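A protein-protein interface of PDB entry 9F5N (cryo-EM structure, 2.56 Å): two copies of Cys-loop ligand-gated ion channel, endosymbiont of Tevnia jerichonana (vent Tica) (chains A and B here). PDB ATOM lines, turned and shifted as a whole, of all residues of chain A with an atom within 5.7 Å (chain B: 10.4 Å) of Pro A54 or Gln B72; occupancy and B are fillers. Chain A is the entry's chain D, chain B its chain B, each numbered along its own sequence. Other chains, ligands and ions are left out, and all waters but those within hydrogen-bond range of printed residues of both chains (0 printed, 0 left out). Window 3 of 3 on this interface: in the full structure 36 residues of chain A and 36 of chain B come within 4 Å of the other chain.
No position is printed for both chains.
Of the 18 printed residues of chain B, 4 touch a printed residue of chain A.
Printed residues of chain A that touch a printed residue of chain B: Pro A54, His A56, Arg A57, Thr A58 and Tyr A59.
Hydrophobic or aromatic side chains of chain A that line the printed part of chain B: Pro A54, His A56 and Tyr A59.
O of Glu B69 is in hydrogen-bond range of NE2 of Gln B72, 3.3 Å away.
No residue of chain B comes within 4 Å of Glu A53.
Pro A54 touches one residue of chain B.
Printed residues of chain B within 4 Å of His A56: Arg B74 (3.3 Å).
Of chain B, only Gln B72 comes within 4 Å of Arg A57.
Of the printed residues of chain B, Tyr A59 touches Glu B69, Gln B72 and Trp B75.
Leu B67 touches none of the printed residues of chain A.
Printed residues of chain A within 4 Å of Glu B69: Thr A58 and Tyr A59.
Of chain A, only Pro A54 (3.4 Å), Arg A57 (3.2 Å) and Tyr A59 (3.9 Å) come within 4 Å of Gln B72.
Printed residues of chain A within 4 Å of Trp B75: Thr A58 (3.8 Å) and Tyr A59 (3.8 Å).
Phe B142 touches none of the printed residues of chain A.
The nearest residue of chain B that does not touch Pro A54 is Ile B73 (5.6 Å).
The nearest printed residue of chain A that does not touch Glu B69 is Arg A57 (7.1 Å).
Among the printed residues, merely in contact across the chains: Pro A54 with Gln B72 (3.4 Å), His A56 with Arg B74 (3.3 Å), Arg A57 with Gln B72 (3.2 Å), Thr A58 with Glu B69 (3.9 Å), Thr A58 with Arg B74 (3.5 Å), Thr A58 with Trp B75 (3.8 Å), Tyr A59 with Glu B69 (3.9 Å), Tyr A59 with Gln B72 (3.9 Å) and Tyr A59 with Trp B75 (3.8 Å).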
ATOM      1  N   PHE A  47      31.923   5.283 -17.116  1.00  0.00           N
ATOM      2  CA  PHE A  47      32.538   5.628 -18.388  1.00  0.00           C
ATOM      3  C   PHE A  47      32.123   7.037 -18.774  1.00  0.00           C
ATOM      4  O   PHE A  47      31.320   7.680 -18.098  1.00  0.00           O
ATOM      5  CB  PHE A  47      32.144   4.636 -19.491  1.00  0.00           C
ATOM      6  CG  PHE A  47      30.668   4.577 -19.755  1.00  0.00           C
ATOM      7  CD1 PHE A  47      29.843   3.779 -18.979  1.00  0.00           C
ATOM      8  CD2 PHE A  47      30.105   5.317 -20.775  1.00  0.00           C
ATOM      9  CE1 PHE A  47      28.497   3.724 -19.220  1.00  0.00           C
ATOM     10  CE2 PHE A  47      28.753   5.260 -21.021  1.00  0.00           C
ATOM     11  CZ  PHE A  47      27.950   4.464 -20.241  1.00  0.00           C
ATOM     12  N   HIS A  49      30.807   8.859 -22.437  1.00  0.00           N
ATOM     13  CA  HIS A  49      30.468   8.648 -23.832  1.00  0.00           C
ATOM     14  C   HIS A  49      31.324   9.547 -24.715  1.00  0.00           C
ATOM     15  O   HIS A  49      31.818  10.594 -24.287  1.00  0.00           O
ATOM     16  CB  HIS A  49      28.983   8.919 -24.069  1.00  0.00           C
ATOM     17  N   ALA A  50      31.506   9.123 -25.958  1.00  0.00           N
ATOM     18  CA  ALA A  50      32.301   9.912 -26.883  1.00  0.00           C
ATOM     19  C   ALA A  50      31.490  11.132 -27.301  1.00  0.00           C
ATOM     20  O   ALA A  50      30.330  11.269 -26.895  1.00  0.00           O
ATOM     21  CB  ALA A  50      32.701   9.076 -28.100  1.00  0.00           C
ATOM     22  N   GLY A  52      28.877  13.214 -28.658  1.00  0.00           N
ATOM     23  CA  GLY A  52      27.592  12.788 -29.177  1.00  0.00           C
ATOM     24  C   GLY A  52      27.503  11.278 -29.253  1.00  0.00           C
ATOM     25  O   GLY A  52      27.272  10.719 -30.330  1.00  0.00           O
ATOM     26  N   GLU A  53      27.720  10.607 -28.125  1.00  0.00           N
ATOM     27  CA  GLU A  53      27.771   9.156 -28.047  1.00  0.00           C
ATOM     28  C   GLU A  53      26.872   8.631 -26.932  1.00  0.00           C
ATOM     29  O   GLU A  53      26.575   9.345 -25.969  1.00  0.00           O
ATOM     30  CB  GLU A  53      29.212   8.674 -27.823  1.00  0.00           C
ATOM     31  N   PRO A  54      26.428   7.375 -27.031  1.00  0.00           N
ATOM     32  CA  PRO A  54      25.363   6.872 -26.146  1.00  0.00           C
ATOM     33  C   PRO A  54      25.668   7.003 -24.659  1.00  0.00           C
ATOM     34  O   PRO A  54      26.726   6.578 -24.190  1.00  0.00           O
ATOM     35  CB  PRO A  54      25.239   5.397 -26.551  1.00  0.00           C
ATOM     36  CG  PRO A  54      26.511   5.081 -27.281  1.00  0.00           C
ATOM     37  CD  PRO A  54      26.910   6.349 -27.964  1.00  0.00           C
ATOM     38  N   LYS A  55      24.735   7.582 -23.907  1.00  0.00           N
ATOM     39  CA  LYS A  55      24.900   7.718 -22.469  1.00  0.00           C
ATOM     40  C   LYS A  55      24.544   6.449 -21.702  1.00  0.00           C
ATOM     41  O   LYS A  55      24.708   6.421 -20.483  1.00  0.00           O
ATOM     42  CB  LYS A  55      24.068   8.893 -21.954  1.00  0.00           C
ATOM     43  CG  LYS A  55      24.301  10.197 -22.706  1.00  0.00           C
ATOM     44  CD  LYS A  55      25.656  10.807 -22.386  1.00  0.00           C
ATOM     45  CE  LYS A  55      25.934  12.053 -23.236  1.00  0.00           C
ATOM     46  NZ  LYS A  55      25.045  13.196 -22.873  1.00  0.00           N
ATOM     47  N   HIS A  56      24.045   5.412 -22.370  1.00  0.00           N
ATOM     48  CA  HIS A  56      23.795   4.128 -21.736  1.00  0.00           C
ATOM     49  C   HIS A  56      24.286   3.020 -22.651  1.00  0.00           C
ATOM     50  O   HIS A  56      24.050   3.053 -23.860  1.00  0.00           O
ATOM     51  CB  HIS A  56      22.315   3.934 -21.418  1.00  0.00           C
ATOM     52  CG  HIS A  56      21.772   4.939 -20.454  1.00  0.00           C
ATOM     53  ND1 HIS A  56      21.541   4.650 -19.128  1.00  0.00           N
ATOM     54  CD2 HIS A  56      21.429   6.238 -20.622  1.00  0.00           C
ATOM     55  CE1 HIS A  56      21.077   5.726 -18.520  1.00  0.00           C
ATOM     56  NE2 HIS A  56      20.997   6.703 -19.404  1.00  0.00           N
ATOM     57  N   ARG A  57      24.976   2.047 -22.078  1.00  0.00           N
ATOM     58  CA  ARG A  57      25.550   0.959 -22.851  1.00  0.00           C
ATOM     59  C   ARG A  57      24.769  -0.321 -22.622  1.00  0.00           C
ATOM     60  O   ARG A  57      24.426  -0.650 -21.486  1.00  0.00           O
ATOM     61  CB  ARG A  57      27.017   0.766 -22.507  1.00  0.00           C
ATOM     62  CG  ARG A  57      27.826   1.943 -22.931  1.00  0.00           C
ATOM     63  CD  ARG A  57      29.248   1.777 -22.546  1.00  0.00           C
ATOM     64  NE  ARG A  57      30.047   2.862 -23.081  1.00  0.00           N
ATOM     65  CZ  ARG A  57      31.337   3.022 -22.846  1.00  0.00           C
ATOM     66  NH1 ARG A  57      32.019   2.148 -22.128  1.00  0.00           N
ATOM     67  NH2 ARG A  57      31.953   4.097 -23.324  1.00  0.00           N
ATOM     68  N   THR A  58      24.477  -1.017 -23.709  1.00  0.00           N
ATOM     69  CA  THR A  58      23.675  -2.228 -23.703  1.00  0.00           C
ATOM     70  C   THR A  58      24.578  -3.437 -23.902  1.00  0.00           C
ATOM     71  O   THR A  58      25.401  -3.457 -24.818  1.00  0.00           O
ATOM     72  CB  THR A  58      22.610  -2.151 -24.795  1.00  0.00           C
ATOM     73  OG1 THR A  58      21.860  -0.941 -24.637  1.00  0.00           O
ATOM     74  CG2 THR A  58      21.664  -3.320 -24.713  1.00  0.00           C
ATOM     75  N   TYR A  59      24.423  -4.437 -23.046  1.00  0.00           N
ATOM     76  CA  TYR A  59      25.251  -5.629 -23.091  1.00  0.00           C
ATOM     77  C   TYR A  59      24.391  -6.879 -23.010  1.00  0.00           C
ATOM     78  O   TYR A  59      23.320  -6.880 -22.405  1.00  0.00           O
ATOM     79  CB  TYR A  59      26.256  -5.646 -21.937  1.00  0.00           C
ATOM     80  CG  TYR A  59      27.369  -4.630 -22.018  1.00  0.00           C
ATOM     81  CD1 TYR A  59      28.464  -4.846 -22.830  1.00  0.00           C
ATOM     82  CD2 TYR A  59      27.324  -3.460 -21.285  1.00  0.00           C
ATOM     83  CE1 TYR A  59      29.479  -3.940 -22.905  1.00  0.00           C
ATOM     84  CE2 TYR A  59      28.342  -2.541 -21.353  1.00  0.00           C
ATOM     85  CZ  TYR A  59      29.415  -2.786 -22.169  1.00  0.00           C
ATOM     86  OH  TYR A  59      30.438  -1.883 -22.249  1.00  0.00           O
ATOM     87  N   TRP B  40      14.983  -3.071 -39.377  1.00  0.00           N
ATOM     88  CA  TRP B  40      15.357  -1.961 -38.507  1.00  0.00           C
ATOM     89  C   TRP B  40      16.525  -1.214 -39.129  1.00  0.00           C
ATOM     90  O   TRP B  40      17.630  -1.748 -39.202  1.00  0.00           O
ATOM     91  CB  TRP B  40      15.695  -2.472 -37.111  1.00  0.00           C
ATOM     92  CG  TRP B  40      16.382  -1.489 -36.225  1.00  0.00           C
ATOM     93  CD1 TRP B  40      15.928  -0.267 -35.852  1.00  0.00           C
ATOM     94  CD2 TRP B  40      17.640  -1.666 -35.568  1.00  0.00           C
ATOM     95  NE1 TRP B  40      16.828   0.339 -35.018  1.00  0.00           N
ATOM     96  CE2 TRP B  40      17.887  -0.504 -34.821  1.00  0.00           C
ATOM     97  CE3 TRP B  40      18.581  -2.695 -35.541  1.00  0.00           C
ATOM     98  CZ2 TRP B  40      19.034  -0.340 -34.061  1.00  0.00           C
ATOM     99  CZ3 TRP B  40      19.718  -2.527 -34.788  1.00  0.00           C
ATOM    100  CH2 TRP B  40      19.935  -1.357 -34.059  1.00  0.00           C
ATOM    101  N   GLN B  42      19.391   1.125 -38.962  1.00  0.00           N
ATOM    102  CA  GLN B  42      20.323   1.792 -38.067  1.00  0.00           C
ATOM    103  C   GLN B  42      21.445   2.407 -38.891  1.00  0.00           C
ATOM    104  O   GLN B  42      22.375   1.690 -39.285  1.00  0.00           O
ATOM    105  CB  GLN B  42      20.875   0.797 -37.044  1.00  0.00           C
ATOM    106  CG  GLN B  42      22.042   1.298 -36.216  1.00  0.00           C
ATOM    107  CD  GLN B  42      21.743   2.566 -35.456  1.00  0.00           C
ATOM    108  OE1 GLN B  42      22.478   3.537 -35.560  1.00  0.00           O
ATOM    109  NE2 GLN B  42      20.689   2.552 -34.659  1.00  0.00           N
ATOM    110  N   LEU B  44      24.085   4.007 -38.250  1.00  0.00           N
ATOM    111  CA  LEU B  44      25.432   3.741 -37.759  1.00  0.00           C
ATOM    112  C   LEU B  44      26.015   2.454 -38.320  1.00  0.00           C
ATOM    113  O   LEU B  44      27.236   2.282 -38.285  1.00  0.00           O
ATOM    114  CB  LEU B  44      25.447   3.675 -36.233  1.00  0.00           C
ATOM    115  CG  LEU B  44      25.328   4.980 -35.456  1.00  0.00           C
ATOM    116  CD1 LEU B  44      25.297   4.684 -33.971  1.00  0.00           C
ATOM    117  CD2 LEU B  44      26.496   5.883 -35.801  1.00  0.00           C
ATOM    118  N   LEU B  45      25.182   1.541 -38.809  1.00  0.00           N
ATOM    119  CA  LEU B  45      25.654   0.284 -39.369  1.00  0.00           C
ATOM    120  C   LEU B  45      26.003   0.372 -40.846  1.00  0.00           C
ATOM    121  O   LEU B  45      26.445  -0.624 -41.420  1.00  0.00           O
ATOM    122  CB  LEU B  45      24.608  -0.810 -39.152  1.00  0.00           C
ATOM    123  CG  LEU B  45      24.460  -1.187 -37.684  1.00  0.00           C
ATOM    124  CD1 LEU B  45      23.396  -2.240 -37.489  1.00  0.00           C
ATOM    125  CD2 LEU B  45      25.798  -1.663 -37.161  1.00  0.00           C
ATOM    126  N   PHE B  64      26.507 -10.616 -35.003  1.00  0.00           N
ATOM    127  CA  PHE B  64      25.883  -9.307 -35.128  1.00  0.00           C
ATOM    128  C   PHE B  64      25.796  -8.599 -33.785  1.00  0.00           C
ATOM    129  O   PHE B  64      26.045  -7.395 -33.704  1.00  0.00           O
ATOM    130  CB  PHE B  64      24.498  -9.432 -35.752  1.00  0.00           C
ATOM    131  CG  PHE B  64      23.865  -8.118 -36.065  1.00  0.00           C
ATOM    132  CD1 PHE B  64      24.421  -7.283 -37.015  1.00  0.00           C
ATOM    133  CD2 PHE B  64      22.719  -7.714 -35.419  1.00  0.00           C
ATOM    134  CE1 PHE B  64      23.847  -6.082 -37.308  1.00  0.00           C
ATOM    135  CE2 PHE B  64      22.146  -6.513 -35.709  1.00  0.00           C
ATOM    136  CZ  PHE B  64      22.710  -5.695 -36.659  1.00  0.00           C
ATOM    137  N   LEU B  65      25.443  -9.323 -32.718  1.00  0.00           N
ATOM    138  CA  LEU B  65      25.355  -8.676 -31.412  1.00  0.00           C
ATOM    139  C   LEU B  65      26.731  -8.266 -30.906  1.00  0.00           C
ATOM    140  O   LEU B  65      26.875  -7.212 -30.282  1.00  0.00           O
ATOM    141  CB  LEU B  65      24.650  -9.580 -30.403  1.00  0.00           C
ATOM    142  CG  LEU B  65      23.127  -9.609 -30.532  1.00  0.00           C
ATOM    143  CD1 LEU B  65      22.493 -10.521 -29.511  1.00  0.00           C
ATOM    144  CD2 LEU B  65      22.537  -8.211 -30.437  1.00  0.00           C
ATOM    145  N   LYS B  66      27.760  -9.070 -31.179  1.00  0.00           N
ATOM    146  CA  LYS B  66      29.114  -8.651 -30.820  1.00  0.00           C
ATOM    147  C   LYS B  66      29.526  -7.396 -31.585  1.00  0.00           C
ATOM    148  O   LYS B  66      30.141  -6.488 -31.018  1.00  0.00           O
ATOM    149  CB  LYS B  66      30.099  -9.794 -31.064  1.00  0.00           C
ATOM    150  CG  LYS B  66      30.208 -10.762 -29.899  1.00  0.00           C
ATOM    151  CD  LYS B  66      30.974 -12.010 -30.288  1.00  0.00           C
ATOM    152  CE  LYS B  66      30.621 -13.164 -29.382  1.00  0.00           C
ATOM    153  NZ  LYS B  66      30.808 -14.476 -30.040  1.00  0.00           N
ATOM    154  N   LEU B  67      29.180  -7.317 -32.869  1.00  0.00           N
ATOM    155  CA  LEU B  67      29.451  -6.115 -33.654  1.00  0.00           C
ATOM    156  C   LEU B  67      28.725  -4.899 -33.082  1.00  0.00           C
ATOM    157  O   LEU B  67      29.293  -3.805 -32.979  1.00  0.00           O
ATOM    158  CB  LEU B  67      29.048  -6.360 -35.110  1.00  0.00           C
ATOM    159  CG  LEU B  67      28.949  -5.194 -36.091  1.00  0.00           C
ATOM    160  CD1 LEU B  67      30.304  -4.589 -36.389  1.00  0.00           C
ATOM    161  CD2 LEU B  67      28.244  -5.615 -37.362  1.00  0.00           C
ATOM    162  N   LEU B  68      27.459  -5.075 -32.704  1.00  0.00           N
ATOM    163  CA  LEU B  68      26.695  -3.984 -32.108  1.00  0.00           C
ATOM    164  C   LEU B  68      27.303  -3.523 -30.791  1.00  0.00           C
ATOM    165  O   LEU B  68      27.357  -2.320 -30.512  1.00  0.00           O
ATOM    166  CB  LEU B  68      25.243  -4.413 -31.918  1.00  0.00           C
ATOM    167  CG  LEU B  68      24.205  -3.786 -32.847  1.00  0.00           C
ATOM    168  CD1 LEU B  68      24.582  -3.949 -34.306  1.00  0.00           C
ATOM    169  CD2 LEU B  68      22.864  -4.386 -32.582  1.00  0.00           C
ATOM    170  N   GLU B  69      27.745  -4.461 -29.957  1.00  0.00           N
ATOM    171  CA  GLU B  69      28.378  -4.087 -28.699  1.00  0.00           C
ATOM    172  C   GLU B  69      29.688  -3.353 -28.942  1.00  0.00           C
ATOM    173  O   GLU B  69      29.996  -2.377 -28.253  1.00  0.00           O
ATOM    174  CB  GLU B  69      28.607  -5.320 -27.831  1.00  0.00           C
ATOM    175  CG  GLU B  69      27.354  -5.863 -27.175  1.00  0.00           C
ATOM    176  CD  GLU B  69      27.468  -7.335 -26.830  1.00  0.00           C
ATOM    177  OE1 GLU B  69      28.250  -8.042 -27.487  1.00  0.00           O
ATOM    178  OE2 GLU B  69      26.780  -7.784 -25.901  1.00  0.00           O
ATOM    179  N   GLU B  70      30.476  -3.811 -29.916  1.00  0.00           N
ATOM    180  CA  GLU B  70      31.730  -3.137 -30.229  1.00  0.00           C
ATOM    181  C   GLU B  70      31.488  -1.714 -30.710  1.00  0.00           C
ATOM    182  O   GLU B  70      32.268  -0.808 -30.404  1.00  0.00           O
ATOM    183  CB  GLU B  70      32.513  -3.930 -31.276  1.00  0.00           C
ATOM    184  N   LYS B  71      30.422  -1.498 -31.474  1.00  0.00           N
ATOM    185  CA  LYS B  71      30.096  -0.159 -31.949  1.00  0.00           C
ATOM    186  C   LYS B  71      29.225   0.615 -30.970  1.00  0.00           C
ATOM    187  O   LYS B  71      28.842   1.747 -31.272  1.00  0.00           O
ATOM    188  CB  LYS B  71      29.400  -0.238 -33.312  1.00  0.00           C
ATOM    189  CG  LYS B  71      30.135  -1.096 -34.314  1.00  0.00           C
ATOM    190  CD  LYS B  71      29.395  -1.191 -35.633  1.00  0.00           C
ATOM    191  CE  LYS B  71      29.350   0.143 -36.343  1.00  0.00           C
ATOM    192  NZ  LYS B  71      30.689   0.638 -36.761  1.00  0.00           N
ATOM    193  N   GLN B  72      28.909   0.033 -29.814  1.00  0.00           N
ATOM    194  CA  GLN B  72      28.072   0.662 -28.791  1.00  0.00           C
ATOM    195  C   GLN B  72      26.726   1.110 -29.358  1.00  0.00           C
ATOM    196  O   GLN B  72      26.277   2.235 -29.151  1.00  0.00           O
ATOM    197  CB  GLN B  72      28.801   1.830 -28.124  1.00  0.00           C
ATOM    198  CG  GLN B  72      30.054   1.441 -27.371  1.00  0.00           C
ATOM    199  CD  GLN B  72      29.783   0.514 -26.198  1.00  0.00           C
ATOM    200  OE1 GLN B  72      28.686   0.496 -25.644  1.00  0.00           O
ATOM    201  NE2 GLN B  72      30.785  -0.261 -25.815  1.00  0.00           N
ATOM    202  N   ILE B  73      26.072   0.210 -30.080  1.00  0.00           N
ATOM    203  CA  ILE B  73      24.750   0.454 -30.643  1.00  0.00           C
ATOM    204  C   ILE B  73      23.745  -0.393 -29.880  1.00  0.00           C
ATOM    205  O   ILE B  73      23.929  -1.607 -29.743  1.00  0.00           O
ATOM    206  CB  ILE B  73      24.720   0.147 -32.150  1.00  0.00           C
ATOM    207  CG1 ILE B  73      25.656   1.098 -32.890  1.00  0.00           C
ATOM    208  CG2 ILE B  73      23.303   0.249 -32.704  1.00  0.00           C
ATOM    209  CD1 ILE B  73      25.849   0.764 -34.319  1.00  0.00           C
ATOM    210  N   ARG B  74      22.694   0.248 -29.376  1.00  0.00           N
ATOM    211  CA  ARG B  74      21.632  -0.448 -28.658  1.00  0.00           C
ATOM    212  C   ARG B  74      20.712  -1.149 -29.651  1.00  0.00           C
ATOM    213  O   ARG B  74      20.236  -0.531 -30.601  1.00  0.00           O
ATOM    214  CB  ARG B  74      20.844   0.535 -27.800  1.00  0.00           C
ATOM    215  CG  ARG B  74      19.617  -0.049 -27.144  1.00  0.00           C
ATOM    216  CD  ARG B  74      18.778   1.015 -26.471  1.00  0.00           C
ATOM    217  NE  ARG B  74      19.417   1.539 -25.275  1.00  0.00           N
ATOM    218  CZ  ARG B  74      19.896   2.768 -25.154  1.00  0.00           C
ATOM    219  NH1 ARG B  74      19.768   3.660 -26.121  1.00  0.00           N
ATOM    220  NH2 ARG B  74      20.516   3.114 -24.033  1.00  0.00           N
ATOM    221  N   TRP B  75      20.476  -2.438 -29.448  1.00  0.00           N
ATOM    222  CA  TRP B  75      19.543  -3.136 -30.309  1.00  0.00           C
ATOM    223  C   TRP B  75      18.128  -3.067 -29.747  1.00  0.00           C
ATOM    224  O   TRP B  75      17.934  -2.894 -28.544  1.00  0.00           O
ATOM    225  CB  TRP B  75      19.979  -4.586 -30.510  1.00  0.00           C
ATOM    226  CG  TRP B  75      20.176  -5.405 -29.267  1.00  0.00           C
ATOM    227  CD1 TRP B  75      19.264  -6.209 -28.671  1.00  0.00           C
ATOM    228  CD2 TRP B  75      21.377  -5.519 -28.495  1.00  0.00           C
ATOM    229  NE1 TRP B  75      19.810  -6.813 -27.570  1.00  0.00           N
ATOM    230  CE2 TRP B  75      21.109  -6.402 -27.437  1.00  0.00           C
ATOM    231  CE3 TRP B  75      22.648  -4.952 -28.591  1.00  0.00           C
ATOM    232  CZ2 TRP B  75      22.064  -6.739 -26.489  1.00  0.00           C
ATOM    233  CZ3 TRP B  75      23.597  -5.289 -27.651  1.00  0.00           C
ATOM    234  CH2 TRP B  75      23.301  -6.169 -26.611  1.00  0.00           C
ATOM    235  N   LEU B 141      12.931   5.473 -27.464  1.00  0.00           N
ATOM    236  CA  LEU B 141      14.073   4.849 -28.119  1.00  0.00           C
ATOM    237  C   LEU B 141      13.664   4.067 -29.361  1.00  0.00           C
ATOM    238  O   LEU B 141      14.211   4.291 -30.442  1.00  0.00           O
ATOM    239  CB  LEU B 141      14.808   3.922 -27.140  1.00  0.00           C
ATOM    240  CG  LEU B 141      15.417   4.530 -25.875  1.00  0.00           C
ATOM    241  CD1 LEU B 141      15.993   3.463 -24.960  1.00  0.00           C
ATOM    242  CD2 LEU B 141      16.469   5.554 -26.230  1.00  0.00           C
ATOM    243  N   PHE B 142      12.703   3.153 -29.229  1.00  0.00           N
ATOM    244  CA  PHE B 142      12.234   2.324 -30.329  1.00  0.00           C
ATOM    245  C   PHE B 142      10.718   2.313 -30.353  1.00  0.00           C
ATOM    246  O   PHE B 142      10.075   2.187 -29.312  1.00  0.00           O
ATOM    247  CB  PHE B 142      12.728   0.871 -30.227  1.00  0.00           C
ATOM    248  CG  PHE B 142      14.211   0.739 -30.165  1.00  0.00           C
ATOM    249  CD1 PHE B 142      14.987   0.973 -31.285  1.00  0.00           C
ATOM    250  CD2 PHE B 142      14.832   0.373 -28.994  1.00  0.00           C
ATOM    251  CE1 PHE B 142      16.338   0.851 -31.232  1.00  0.00           C
ATOM    252  CE2 PHE B 142      16.191   0.252 -28.940  1.00  0.00           C
ATOM    253  CZ  PHE B 142      16.945   0.492 -30.062  1.00  0.00           C
